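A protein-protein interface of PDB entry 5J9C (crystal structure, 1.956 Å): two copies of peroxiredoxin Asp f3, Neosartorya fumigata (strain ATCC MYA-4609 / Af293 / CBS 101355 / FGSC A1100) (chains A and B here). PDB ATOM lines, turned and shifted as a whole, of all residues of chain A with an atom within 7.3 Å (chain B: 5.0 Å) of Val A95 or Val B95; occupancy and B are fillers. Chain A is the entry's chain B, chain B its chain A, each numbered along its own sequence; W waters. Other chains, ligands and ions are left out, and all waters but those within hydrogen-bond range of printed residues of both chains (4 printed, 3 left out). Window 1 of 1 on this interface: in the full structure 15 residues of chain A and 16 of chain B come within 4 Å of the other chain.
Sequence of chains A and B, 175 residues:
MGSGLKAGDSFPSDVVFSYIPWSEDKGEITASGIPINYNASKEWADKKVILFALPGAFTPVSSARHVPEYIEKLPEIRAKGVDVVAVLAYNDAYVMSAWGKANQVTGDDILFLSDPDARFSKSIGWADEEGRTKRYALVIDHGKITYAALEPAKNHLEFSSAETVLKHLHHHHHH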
ATOM      1  N   ILE A  20       7.442 -29.005  25.633  1.00  0.00           N
ATOM      2  CA  ILE A  20       8.387 -30.104  25.709  1.00  0.00           C
ATOM      3  C   ILE A  20       8.126 -30.821  27.014  1.00  0.00           C
ATOM      4  O   ILE A  20       8.321 -30.238  28.075  1.00  0.00           O
ATOM      5  CB  ILE A  20       9.856 -29.626  25.668  1.00  0.00           C
ATOM      6  CG1 ILE A  20      10.157 -28.914  24.347  1.00  0.00           C
ATOM      7  CG2 ILE A  20      10.806 -30.802  25.904  1.00  0.00           C
ATOM      8  CD1 ILE A  20      11.539 -28.275  24.280  1.00  0.00           C
ATOM      9  N   ILE A  29      19.152 -27.585  32.290  1.00  0.00           N
ATOM     10  CA  ILE A  29      18.507 -26.484  31.598  1.00  0.00           C
ATOM     11  C   ILE A  29      19.193 -26.241  30.240  1.00  0.00           C
ATOM     12  O   ILE A  29      18.562 -25.773  29.293  1.00  0.00           O
ATOM     13  CB  ILE A  29      18.506 -25.205  32.464  1.00  0.00           C
ATOM     14  CG1 ILE A  29      17.586 -24.140  31.853  1.00  0.00           C
ATOM     15  CG2 ILE A  29      19.931 -24.697  32.718  1.00  0.00           C
ATOM     16  CD1 ILE A  29      17.419 -22.926  32.741  1.00  0.00           C
ATOM     17  N   GLY A  56       5.323 -13.385  30.414  1.00  0.00           N
ATOM     18  CA  GLY A  56       6.366 -14.175  29.799  1.00  0.00           C
ATOM     19  C   GLY A  56       7.259 -14.929  30.757  1.00  0.00           C
ATOM     20  O   GLY A  56       7.392 -14.565  31.936  1.00  0.00           O
ATOM     21  N   ALA A  57       7.874 -15.992  30.240  1.00  0.00           N
ATOM     22  CA  ALA A  57       8.928 -16.688  30.971  1.00  0.00           C
ATOM     23  C   ALA A  57      10.025 -15.713  31.397  1.00  0.00           C
ATOM     24  O   ALA A  57      10.373 -14.792  30.646  1.00  0.00           O
ATOM     25  CB  ALA A  57       9.523 -17.804  30.118  1.00  0.00           C
ATOM     26  N   PHE A  58      10.546 -15.920  32.606  1.00  0.00           N
ATOM     27  CA  PHE A  58      11.666 -15.132  33.139  1.00  0.00           C
ATOM     28  C   PHE A  58      11.389 -13.618  33.283  1.00  0.00           C
ATOM     29  O   PHE A  58      12.333 -12.822  33.341  1.00  0.00           O
ATOM     30  CB  PHE A  58      12.916 -15.345  32.268  1.00  0.00           C
ATOM     31  CG  PHE A  58      13.344 -16.788  32.156  1.00  0.00           C
ATOM     32  CD1 PHE A  58      13.970 -17.431  33.220  1.00  0.00           C
ATOM     33  CD2 PHE A  58      13.138 -17.496  30.980  1.00  0.00           C
ATOM     34  CE1 PHE A  58      14.370 -18.762  33.118  1.00  0.00           C
ATOM     35  CE2 PHE A  58      13.535 -18.826  30.870  1.00  0.00           C
ATOM     36  CZ  PHE A  58      14.158 -19.458  31.941  1.00  0.00           C
ATOM     37  N   THR A  59      10.115 -13.223  33.371  1.00  0.00           N
ATOM     38  CA  THR A  59       9.746 -11.826  33.678  1.00  0.00           C
ATOM     39  C   THR A  59       9.649 -11.646  35.209  1.00  0.00           C
ATOM     40  O   THR A  59       9.482 -12.630  35.913  1.00  0.00           O
ATOM     41  CB  THR A  59       8.410 -11.436  32.998  1.00  0.00           C
ATOM     42  OG1 THR A  59       7.427 -12.441  33.271  1.00  0.00           O
ATOM     43  CG2 THR A  59       8.580 -11.300  31.480  1.00  0.00           C
ATOM     44  N   TYR A  90       3.566 -16.569  25.954  1.00  0.00           N
ATOM     45  CA  TYR A  90       3.739 -16.493  24.509  1.00  0.00           C
ATOM     46  C   TYR A  90       5.091 -17.046  24.051  1.00  0.00           C
ATOM     47  O   TYR A  90       5.302 -17.220  22.855  1.00  0.00           O
ATOM     48  CB  TYR A  90       3.554 -15.040  24.029  1.00  0.00           C
ATOM     49  CG  TYR A  90       4.776 -14.143  24.162  1.00  0.00           C
ATOM     50  CD1 TYR A  90       5.125 -13.271  23.131  1.00  0.00           C
ATOM     51  CD2 TYR A  90       5.572 -14.155  25.310  1.00  0.00           C
ATOM     52  CE1 TYR A  90       6.241 -12.442  23.226  1.00  0.00           C
ATOM     53  CE2 TYR A  90       6.708 -13.323  25.414  1.00  0.00           C
ATOM     54  CZ  TYR A  90       7.028 -12.474  24.366  1.00  0.00           C
ATOM     55  OH  TYR A  90       8.139 -11.650  24.444  1.00  0.00           O
ATOM     56  N   ASN A  91       6.003 -17.325  24.984  1.00  0.00           N
ATOM     57  CA  ASN A  91       7.340 -17.822  24.609  1.00  0.00           C
ATOM     58  C   ASN A  91       7.241 -19.199  23.953  1.00  0.00           C
ATOM     59  O   ASN A  91       6.250 -19.904  24.170  1.00  0.00           O
ATOM     60  CB  ASN A  91       8.271 -17.907  25.821  1.00  0.00           C
ATOM     61  CG  ASN A  91       8.238 -16.652  26.674  1.00  0.00           C
ATOM     62  OD1 ASN A  91       7.382 -16.509  27.537  1.00  0.00           O
ATOM     63  ND2 ASN A  91       9.161 -15.729  26.418  1.00  0.00           N
ATOM     64  N   ASP A  92       8.246 -19.587  23.167  1.00  0.00           N
ATOM     65  CA  ASP A  92       8.183 -20.890  22.488  1.00  0.00           C
ATOM     66  C   ASP A  92       8.444 -22.035  23.481  1.00  0.00           C
ATOM     67  O   ASP A  92       8.817 -21.793  24.625  1.00  0.00           O
ATOM     68  CB  ASP A  92       9.154 -20.951  21.282  1.00  0.00           C
ATOM     69  CG  ASP A  92      10.646 -20.958  21.677  1.00  0.00           C
ATOM     70  OD1 ASP A  92      11.019 -21.512  22.735  1.00  0.00           O
ATOM     71  OD2 ASP A  92      11.471 -20.432  20.883  1.00  0.00           O
ATOM     72  N   ALA A  93       8.249 -23.278  23.038  1.00  0.00           N
ATOM     73  CA  ALA A  93       8.314 -24.431  23.942  1.00  0.00           C
ATOM     74  C   ALA A  93       9.712 -24.649  24.523  1.00  0.00           C
ATOM     75  O   ALA A  93       9.850 -25.117  25.652  1.00  0.00           O
ATOM     76  CB  ALA A  93       7.844 -25.692  23.219  1.00  0.00           C
ATOM     77  N   TYR A  94      10.749 -24.323  23.755  1.00  0.00           N
ATOM     78  CA  TYR A  94      12.125 -24.431  24.260  1.00  0.00           C
ATOM     79  C   TYR A  94      12.324 -23.556  25.500  1.00  0.00           C
ATOM     80  O   TYR A  94      12.914 -23.983  26.496  1.00  0.00           O
ATOM     81  CB  TYR A  94      13.152 -24.029  23.190  1.00  0.00           C
ATOM     82  CG  TYR A  94      13.155 -24.888  21.949  1.00  0.00           C
ATOM     83  CD1 TYR A  94      13.706 -26.160  21.963  1.00  0.00           C
ATOM     84  CD2 TYR A  94      12.625 -24.412  20.750  1.00  0.00           C
ATOM     85  CE1 TYR A  94      13.712 -26.951  20.822  1.00  0.00           C
ATOM     86  CE2 TYR A  94      12.626 -25.194  19.603  1.00  0.00           C
ATOM     87  CZ  TYR A  94      13.170 -26.459  19.643  1.00  0.00           C
ATOM     88  OH  TYR A  94      13.169 -27.233  18.500  1.00  0.00           O
ATOM     89  N   VAL A  95      11.843 -22.320  25.420  1.00  0.00           N
ATOM     90  CA  VAL A  95      11.950 -21.379  26.525  1.00  0.00           C
ATOM     91  C   VAL A  95      11.075 -21.788  27.713  1.00  0.00           C
ATOM     92  O   VAL A  95      11.521 -21.740  28.857  1.00  0.00           O
ATOM     93  CB  VAL A  95      11.569 -19.952  26.068  1.00  0.00           C
ATOM     94  CG1 VAL A  95      11.541 -18.991  27.257  1.00  0.00           C
ATOM     95  CG2 VAL A  95      12.538 -19.470  24.981  1.00  0.00           C
ATOM     96  N   MET A  96       9.837 -22.192  27.452  1.00  0.00           N
ATOM     97  CA  MET A  96       8.963 -22.603  28.551  1.00  0.00           C
ATOM     98  C   MET A  96       9.559 -23.817  29.269  1.00  0.00           C
ATOM     99  O   MET A  96       9.505 -23.896  30.493  1.00  0.00           O
ATOM    100  CB  MET A  96       7.551 -22.911  28.055  1.00  0.00           C
ATOM    101  CG  MET A  96       6.782 -21.678  27.525  1.00  0.00           C
ATOM    102  SD  MET A  96       6.650 -20.308  28.720  1.00  0.00           S
ATOM    103  CE  MET A  96       5.589 -21.035  29.976  1.00  0.00           C
ATOM    104  N   SER A  97      10.143 -24.741  28.505  1.00  0.00           N
ATOM    105  CA  SER A  97      10.783 -25.933  29.069  1.00  0.00           C
ATOM    106  C   SER A  97      11.924 -25.547  30.002  1.00  0.00           C
ATOM    107  O   SER A  97      12.018 -26.033  31.135  1.00  0.00           O
ATOM    108  CB  SER A  97      11.301 -26.837  27.949  1.00  0.00           C
ATOM    109  OG  SER A  97      11.965 -27.990  28.456  1.00  0.00           O
ATOM    110  N   ALA A  98      12.784 -24.658  29.512  1.00  0.00           N
ATOM    111  CA  ALA A  98      13.919 -24.170  30.279  1.00  0.00           C
ATOM    112  C   ALA A  98      13.460 -23.490  31.571  1.00  0.00           C
ATOM    113  O   ALA A  98      14.091 -23.630  32.622  1.00  0.00           O
ATOM    114  CB  ALA A  98      14.746 -23.204  29.432  1.00  0.00           C
ATOM    115  N   TRP A  99      12.352 -22.763  31.482  1.00  0.00           N
ATOM    116  CA  TRP A  99      11.813 -22.042  32.629  1.00  0.00           C
ATOM    117  C   TRP A  99      11.342 -23.011  33.706  1.00  0.00           C
ATOM    118  O   TRP A  99      11.530 -22.761  34.896  1.00  0.00           O
ATOM    119  CB  TRP A  99      10.655 -21.145  32.206  1.00  0.00           C
ATOM    120  CG  TRP A  99      10.315 -20.055  33.199  1.00  0.00           C
ATOM    121  CD1 TRP A  99      11.164 -19.449  34.099  1.00  0.00           C
ATOM    122  CD2 TRP A  99       9.038 -19.432  33.371  1.00  0.00           C
ATOM    123  NE1 TRP A  99      10.480 -18.492  34.817  1.00  0.00           N
ATOM    124  CE2 TRP A  99       9.176 -18.460  34.385  1.00  0.00           C
ATOM    125  CE3 TRP A  99       7.786 -19.602  32.760  1.00  0.00           C
ATOM    126  CZ2 TRP A  99       8.105 -17.663  34.809  1.00  0.00           C
ATOM    127  CZ3 TRP A  99       6.725 -18.801  33.172  1.00  0.00           C
ATOM    128  CH2 TRP A  99       6.891 -17.847  34.190  1.00  0.00           C
ATOM    129  N   GLY A 100      10.730 -24.113  33.279  1.00  0.00           N
ATOM    130  CA  GLY A 100      10.311 -25.148  34.209  1.00  0.00           C
ATOM    131  C   GLY A 100      11.507 -25.673  34.987  1.00  0.00           C
ATOM    132  O   GLY A 100      11.461 -25.831  36.218  1.00  0.00           O
ATOM    133  N   LYS A 101      12.594 -25.926  34.264  1.00  0.00           N
ATOM    134  CA  LYS A 101      13.832 -26.397  34.877  1.00  0.00           C
ATOM    135  C   LYS A 101      14.458 -25.353  35.789  1.00  0.00           C
ATOM    136  O   LYS A 101      14.991 -25.696  36.847  1.00  0.00           O
ATOM    137  CB  LYS A 101      14.830 -26.806  33.801  1.00  0.00           C
ATOM    138  CG  LYS A 101      14.357 -27.990  32.964  1.00  0.00           C
ATOM    139  CD  LYS A 101      15.180 -28.098  31.693  1.00  0.00           C
ATOM    140  CE  LYS A 101      14.493 -29.010  30.674  1.00  0.00           C
ATOM    141  NZ  LYS A 101      15.274 -29.049  29.405  1.00  0.00           N
ATOM    142  N   PHE A 112       4.613 -26.518  31.626  1.00  0.00           N
ATOM    143  CA  PHE A 112       5.069 -25.224  31.127  1.00  0.00           C
ATOM    144  C   PHE A 112       4.791 -25.156  29.643  1.00  0.00           C
ATOM    145  O   PHE A 112       5.529 -25.719  28.830  1.00  0.00           O
ATOM    146  CB  PHE A 112       6.551 -25.012  31.439  1.00  0.00           C
ATOM    147  CG  PHE A 112       6.806 -24.639  32.881  1.00  0.00           C
ATOM    148  CD1 PHE A 112       6.557 -25.550  33.894  1.00  0.00           C
ATOM    149  CD2 PHE A 112       7.291 -23.377  33.214  1.00  0.00           C
ATOM    150  CE1 PHE A 112       6.779 -25.213  35.231  1.00  0.00           C
ATOM    151  CE2 PHE A 112       7.515 -23.027  34.546  1.00  0.00           C
ATOM    152  CZ  PHE A 112       7.257 -23.942  35.554  1.00  0.00           C
ATOM    153  N   ARG A 132       1.954 -10.499  23.697  1.00  0.00           N
ATOM    154  CA  ARG A 132       2.090 -11.320  24.902  1.00  0.00           C
ATOM    155  C   ARG A 132       0.723 -11.744  25.434  1.00  0.00           C
ATOM    156  O   ARG A 132      -0.269 -11.035  25.232  1.00  0.00           O
ATOM    157  CB  ARG A 132       2.844 -10.553  25.994  1.00  0.00           C
ATOM    158  CG  ARG A 132       4.286 -10.197  25.653  1.00  0.00           C
ATOM    159  CD  ARG A 132       4.889  -9.383  26.803  1.00  0.00           C
ATOM    160  NE  ARG A 132       6.280  -9.008  26.569  1.00  0.00           N
ATOM    161  CZ  ARG A 132       7.336  -9.703  26.996  1.00  0.00           C
ATOM    162  NH1 ARG A 132       7.168 -10.828  27.694  1.00  0.00           N
ATOM    163  NH2 ARG A 132       8.566  -9.262  26.724  1.00  0.00           N
ATOM    164  N   ALA B  57      17.215 -18.873  21.939  1.00  0.00           N
ATOM    165  CA  ALA B  57      17.694 -19.296  23.237  1.00  0.00           C
ATOM    166  C   ALA B  57      17.156 -20.690  23.563  1.00  0.00           C
ATOM    167  O   ALA B  57      16.010 -21.015  23.237  1.00  0.00           O
ATOM    168  CB  ALA B  57      17.265 -18.294  24.314  1.00  0.00           C
ATOM    169  N   PHE B  58      17.993 -21.501  24.200  1.00  0.00           N
ATOM    170  CA  PHE B  58      17.596 -22.813  24.720  1.00  0.00           C
ATOM    171  C   PHE B  58      17.220 -23.799  23.609  1.00  0.00           C
ATOM    172  O   PHE B  58      16.481 -24.751  23.851  1.00  0.00           O
ATOM    173  CB  PHE B  58      16.435 -22.679  25.731  1.00  0.00           C
ATOM    174  CG  PHE B  58      16.779 -21.833  26.939  1.00  0.00           C
ATOM    175  CD1 PHE B  58      17.682 -22.295  27.886  1.00  0.00           C
ATOM    176  CD2 PHE B  58      16.208 -20.575  27.118  1.00  0.00           C
ATOM    177  CE1 PHE B  58      18.009 -21.518  29.005  1.00  0.00           C
ATOM    178  CE2 PHE B  58      16.522 -19.796  28.228  1.00  0.00           C
ATOM    179  CZ  PHE B  58      17.426 -20.266  29.174  1.00  0.00           C
ATOM    180  N   ASN B  91      14.318 -13.971  20.707  1.00  0.00           N
ATOM    181  CA  ASN B  91      13.666 -14.029  22.026  1.00  0.00           C
ATOM    182  C   ASN B  91      13.731 -12.671  22.702  1.00  0.00           C
ATOM    183  O   ASN B  91      14.631 -11.884  22.409  1.00  0.00           O
ATOM    184  CB  ASN B  91      14.328 -15.092  22.921  1.00  0.00           C
ATOM    185  CG  ASN B  91      14.459 -16.440  22.229  1.00  0.00           C
ATOM    186  OD1 ASN B  91      15.417 -16.687  21.491  1.00  0.00           O
ATOM    187  ND2 ASN B  91      13.499 -17.323  22.473  1.00  0.00           N
ATOM    188  N   ASP B  92      12.802 -12.383  23.612  1.00  0.00           N
ATOM    189  CA  ASP B  92      12.803 -11.054  24.224  1.00  0.00           C
ATOM    190  C   ASP B  92      13.982 -10.989  25.195  1.00  0.00           C
ATOM    191  O   ASP B  92      14.660 -11.994  25.423  1.00  0.00           O
ATOM    192  CB  ASP B  92      11.444 -10.712  24.895  1.00  0.00           C
ATOM    193  CG  ASP B  92      11.135 -11.548  26.149  1.00  0.00           C
ATOM    194  OD1 ASP B  92      12.054 -12.034  26.840  1.00  0.00           O
ATOM    195  OD2 ASP B  92       9.925 -11.695  26.460  1.00  0.00           O
ATOM    196  N   ALA B  93      14.233  -9.811  25.756  1.00  0.00           N
ATOM    197  CA  ALA B  93      15.440  -9.604  26.542  1.00  0.00           C
ATOM    198  C   ALA B  93      15.419 -10.378  27.863  1.00  0.00           C
ATOM    199  O   ALA B  93      16.477 -10.718  28.404  1.00  0.00           O
ATOM    200  CB  ALA B  93      15.646  -8.112  26.804  1.00  0.00           C
ATOM    201  N   TYR B  94      14.227 -10.642  28.388  1.00  0.00           N
ATOM    202  CA  TYR B  94      14.102 -11.428  29.617  1.00  0.00           C
ATOM    203  C   TYR B  94      14.650 -12.827  29.403  1.00  0.00           C
ATOM    204  O   TYR B  94      15.373 -13.370  30.236  1.00  0.00           O
ATOM    205  CB  TYR B  94      12.641 -11.530  30.069  1.00  0.00           C
ATOM    206  CG  TYR B  94      11.997 -10.211  30.414  1.00  0.00           C
ATOM    207  CD1 TYR B  94      12.260  -9.584  31.623  1.00  0.00           C
ATOM    208  CD2 TYR B  94      11.092  -9.609  29.543  1.00  0.00           C
ATOM    209  CE1 TYR B  94      11.656  -8.383  31.945  1.00  0.00           C
ATOM    210  CE2 TYR B  94      10.481  -8.413  29.856  1.00  0.00           C
ATOM    211  CZ  TYR B  94      10.762  -7.804  31.051  1.00  0.00           C
ATOM    212  OH  TYR B  94      10.153  -6.611  31.360  1.00  0.00           O
ATOM    213  N   VAL B  95      14.269 -13.418  28.277  1.00  0.00           N
ATOM    214  CA  VAL B  95      14.714 -14.763  27.931  1.00  0.00           C
ATOM    215  C   VAL B  95      16.212 -14.800  27.605  1.00  0.00           C
ATOM    216  O   VAL B  95      16.922 -15.694  28.062  1.00  0.00           O
ATOM    217  CB  VAL B  95      13.898 -15.318  26.740  1.00  0.00           C
ATOM    218  CG1 VAL B  95      14.446 -16.646  26.280  1.00  0.00           C
ATOM    219  CG2 VAL B  95      12.418 -15.447  27.137  1.00  0.00           C
ATOM    220  N   MET B  96      16.698 -13.831  26.826  1.00  0.00           N
ATOM    221  CA  MET B  96      18.126 -13.789  26.501  1.00  0.00           C
ATOM    222  C   MET B  96      18.969 -13.629  27.779  1.00  0.00           C
ATOM    223  O   MET B  96      20.023 -14.253  27.937  1.00  0.00           O
ATOM    224  CB  MET B  96      18.425 -12.654  25.511  1.00  0.00           C
ATOM    225  CG  MET B  96      17.826 -12.870  24.105  1.00  0.00           C
ATOM    226  SD  MET B  96      18.342 -14.448  23.369  1.00  0.00           S
ATOM    227  CE  MET B  96      20.087 -14.143  23.058  1.00  0.00           C
ATOM    228  N   SER B  97      18.499 -12.777  28.683  1.00  0.00           N
ATOM    229  CA  SER B  97      19.168 -12.574  29.963  1.00  0.00           C
ATOM    230  C   SER B  97      19.283 -13.877  30.760  1.00  0.00           C
ATOM    231  O   SER B  97      20.360 -14.228  31.253  1.00  0.00           O
ATOM    232  CB  SER B  97      18.419 -11.519  30.779  1.00  0.00           C
ATOM    233  OG  SER B  97      18.963 -11.384  32.082  1.00  0.00           O
ATOM    234  N   ALA B  98      18.172 -14.601  30.867  1.00  0.00           N
ATOM    235  CA  ALA B  98      18.160 -15.872  31.580  1.00  0.00           C
ATOM    236  C   ALA B  98      19.083 -16.892  30.924  1.00  0.00           C
ATOM    237  O   ALA B  98      19.747 -17.674  31.613  1.00  0.00           O
ATOM    238  CB  ALA B  98      16.755 -16.419  31.657  1.00  0.00           C
ATOM    239  N   TRP B  99      19.120 -16.886  29.594  1.00  0.00           N
ATOM    240  CA  TRP B  99      19.967 -17.820  28.864  1.00  0.00           C
ATOM    241  C   TRP B  99      21.441 -17.564  29.188  1.00  0.00           C
ATOM    242  O   TRP B  99      22.235 -18.499  29.318  1.00  0.00           O
ATOM    243  CB  TRP B  99      19.721 -17.694  27.360  1.00  0.00           C
ATOM    244  CG  TRP B  99      20.219 -18.865  26.542  1.00  0.00           C
ATOM    245  CD1 TRP B  99      20.316 -20.174  26.943  1.00  0.00           C
ATOM    246  CD2 TRP B  99      20.678 -18.826  25.186  1.00  0.00           C
ATOM    247  NE1 TRP B  99      20.800 -20.953  25.909  1.00  0.00           N
ATOM    248  CE2 TRP B  99      21.035 -20.147  24.823  1.00  0.00           C
ATOM    249  CE3 TRP B  99      20.810 -17.803  24.235  1.00  0.00           C
ATOM    250  CZ2 TRP B  99      21.517 -20.468  23.553  1.00  0.00           C
ATOM    251  CZ3 TRP B  99      21.291 -18.127  22.973  1.00  0.00           C
ATOM    252  CH2 TRP B  99      21.639 -19.445  22.645  1.00  0.00           C
HETATM  253  O   HOH W   1      15.242 -12.706  32.976  1.00  0.00           O
HETATM  254  O   HOH W   2       9.249 -13.499  28.314  1.00  0.00           O
HETATM  255  O   HOH W   3      14.817 -25.974  26.205  1.00  0.00           O
HETATM  256  O   HOH W   4      14.011 -19.977  21.286  1.00  0.00           O
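The side-chain carboxylate (OD2) of Asp B92 sits at hydrogen-bond distance from the side-chain hydroxyl (OH) of Tyr A90 (2.7 Å).
The side-chain carboxylate (OD2) of Asp B92 is in salt-bridge range of the guanidinium group (NH2) of Arg A132, 2.8 Å away.
N of Ala A57 sits at hydrogen-bond distance from OD1 of Asn A91 (2.8 Å).
The side-chain carboxylate (OD1) of Asp B92 sits at hydrogen-bond distance from the backbone NH (N) of Val B95, 3.0 Å away.
N of Tyr B94 lies within hydrogen-bond range of OD1 of Asp B92, 3.0 Å away.
O of Gly A56 is in hydrogen-bond range of OG1 of Thr A59 (2.5 Å).
OD1 of Asp A92 sits at hydrogen-bond distance from N of Tyr A94, at 3.0 Å.
The guanidinium group of Arg A132 sits close to the side-chain hydroxyl of Tyr A90, at 3.3 Å.
Among the printed residues, pairs that only touch across the chains: Ile A29 with Phe B58 (3.9 Å), Phe A58 with Tyr B94 (3.5 Å), Phe A58 with Ala B98 (3.4 Å), Thr A59 with Tyr B94 (3.6 Å), Asn A91 with Val B95 (3.3 Å), Tyr A94 with Phe B58 (3.5 Å), Val A95 with Asn B91 (3.4 Å), Val A95 with Val B95 (3.6 Å), Ala A98 with Phe B58 (3.4 Å) and Arg A132 with Tyr B94 (3.8 Å).
Of chain B, only Asn B91 and Val B95 come within 4 Å of Val A95.
Printed residues of chain A within 4 Å of Val B95: Asn A91 (3.3 Å) and Val A95 (3.6 Å).
Of the printed residues of chain A, Asn B91 touches Val A95 (3.4 Å).
Of the printed residues of chain B, Asn A91 touches Val B95.
Of the printed residues of chain A, Asp B92 touches Tyr A90 (2.7 Å) and Arg A132 (2.8 Å).
Of the printed residues of chain B, Arg A132 touches Asp B92 and Tyr B94.
Printed residues of chain B within 4 Å of Tyr A94: Phe B58 (3.5 Å).
Ala A93 touches none of the printed residues of chain B.
Ala B57 touches none of the printed residues of chain A.
The nearest residue of chain B that does not touch Val A95 is Ala B57 (4.2 Å).
The nearest residue of chain A that does not touch Val B95 is Ala A57 (4.1 Å).
The nearest printed residue of chain B that does not touch Tyr A94 is Ala B57 (4.2 Å).
Hydrophobic or aromatic side chains of chain B that line the printed part of chain A: Phe B58, Tyr B94, Val B95 and Ala B98.
Among the printed residues, Asp or Glu carboxylates within 4 Å of a Lys or Arg side-chain nitrogen of the other chain: Arg A132 with Asp B92.
Phe A58 touches Tyr B94, and with the chains exchanged Tyr A94 touches Phe B58.
Phe A58 touches Ala B98, and with the chains exchanged Ala A98 touches Phe B58.
Asn A91 touches Val B95, and with the chains exchanged Val A95 touches Asn B91.
Val A95 touches its own counterpart, Val B95.
Positions printed for both chains: 57, 58, 91, 92, 93, 94, 95, 96, 97, 98 and 99.
Of the 12 pairs that touch across the chains among the printed residues, 7 have their exchanged pair printed and touching as well.
Water W4 lies within hydrogen-bond range of the side-chain carboxylate (OD2) of Asp A92, the side-chain amide nitrogen (ND2) of Asn B91 and the backbone carbonyl oxygen (O) of Ala B57.
Water W2 lies within hydrogen-bond range of OD2 of Asp B92 (2.7 Å), O of Ala A57 (2.9 Å), ND2 of Asn A91 (2.9 Å) and NH1 of Arg A132 (3.4 Å).
Water W3 bridges the backbone carbonyl oxygen (O) of Tyr A94 (2.8 Å) and the backbone carbonyl oxygen (O) of Phe B58 (3.1 Å).
Water W1 lies within hydrogen-bond range of the backbone carbonyl oxygen of Tyr B94 (2.8 Å) and the backbone carbonyl oxygen of Phe A58 (2.9 Å).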
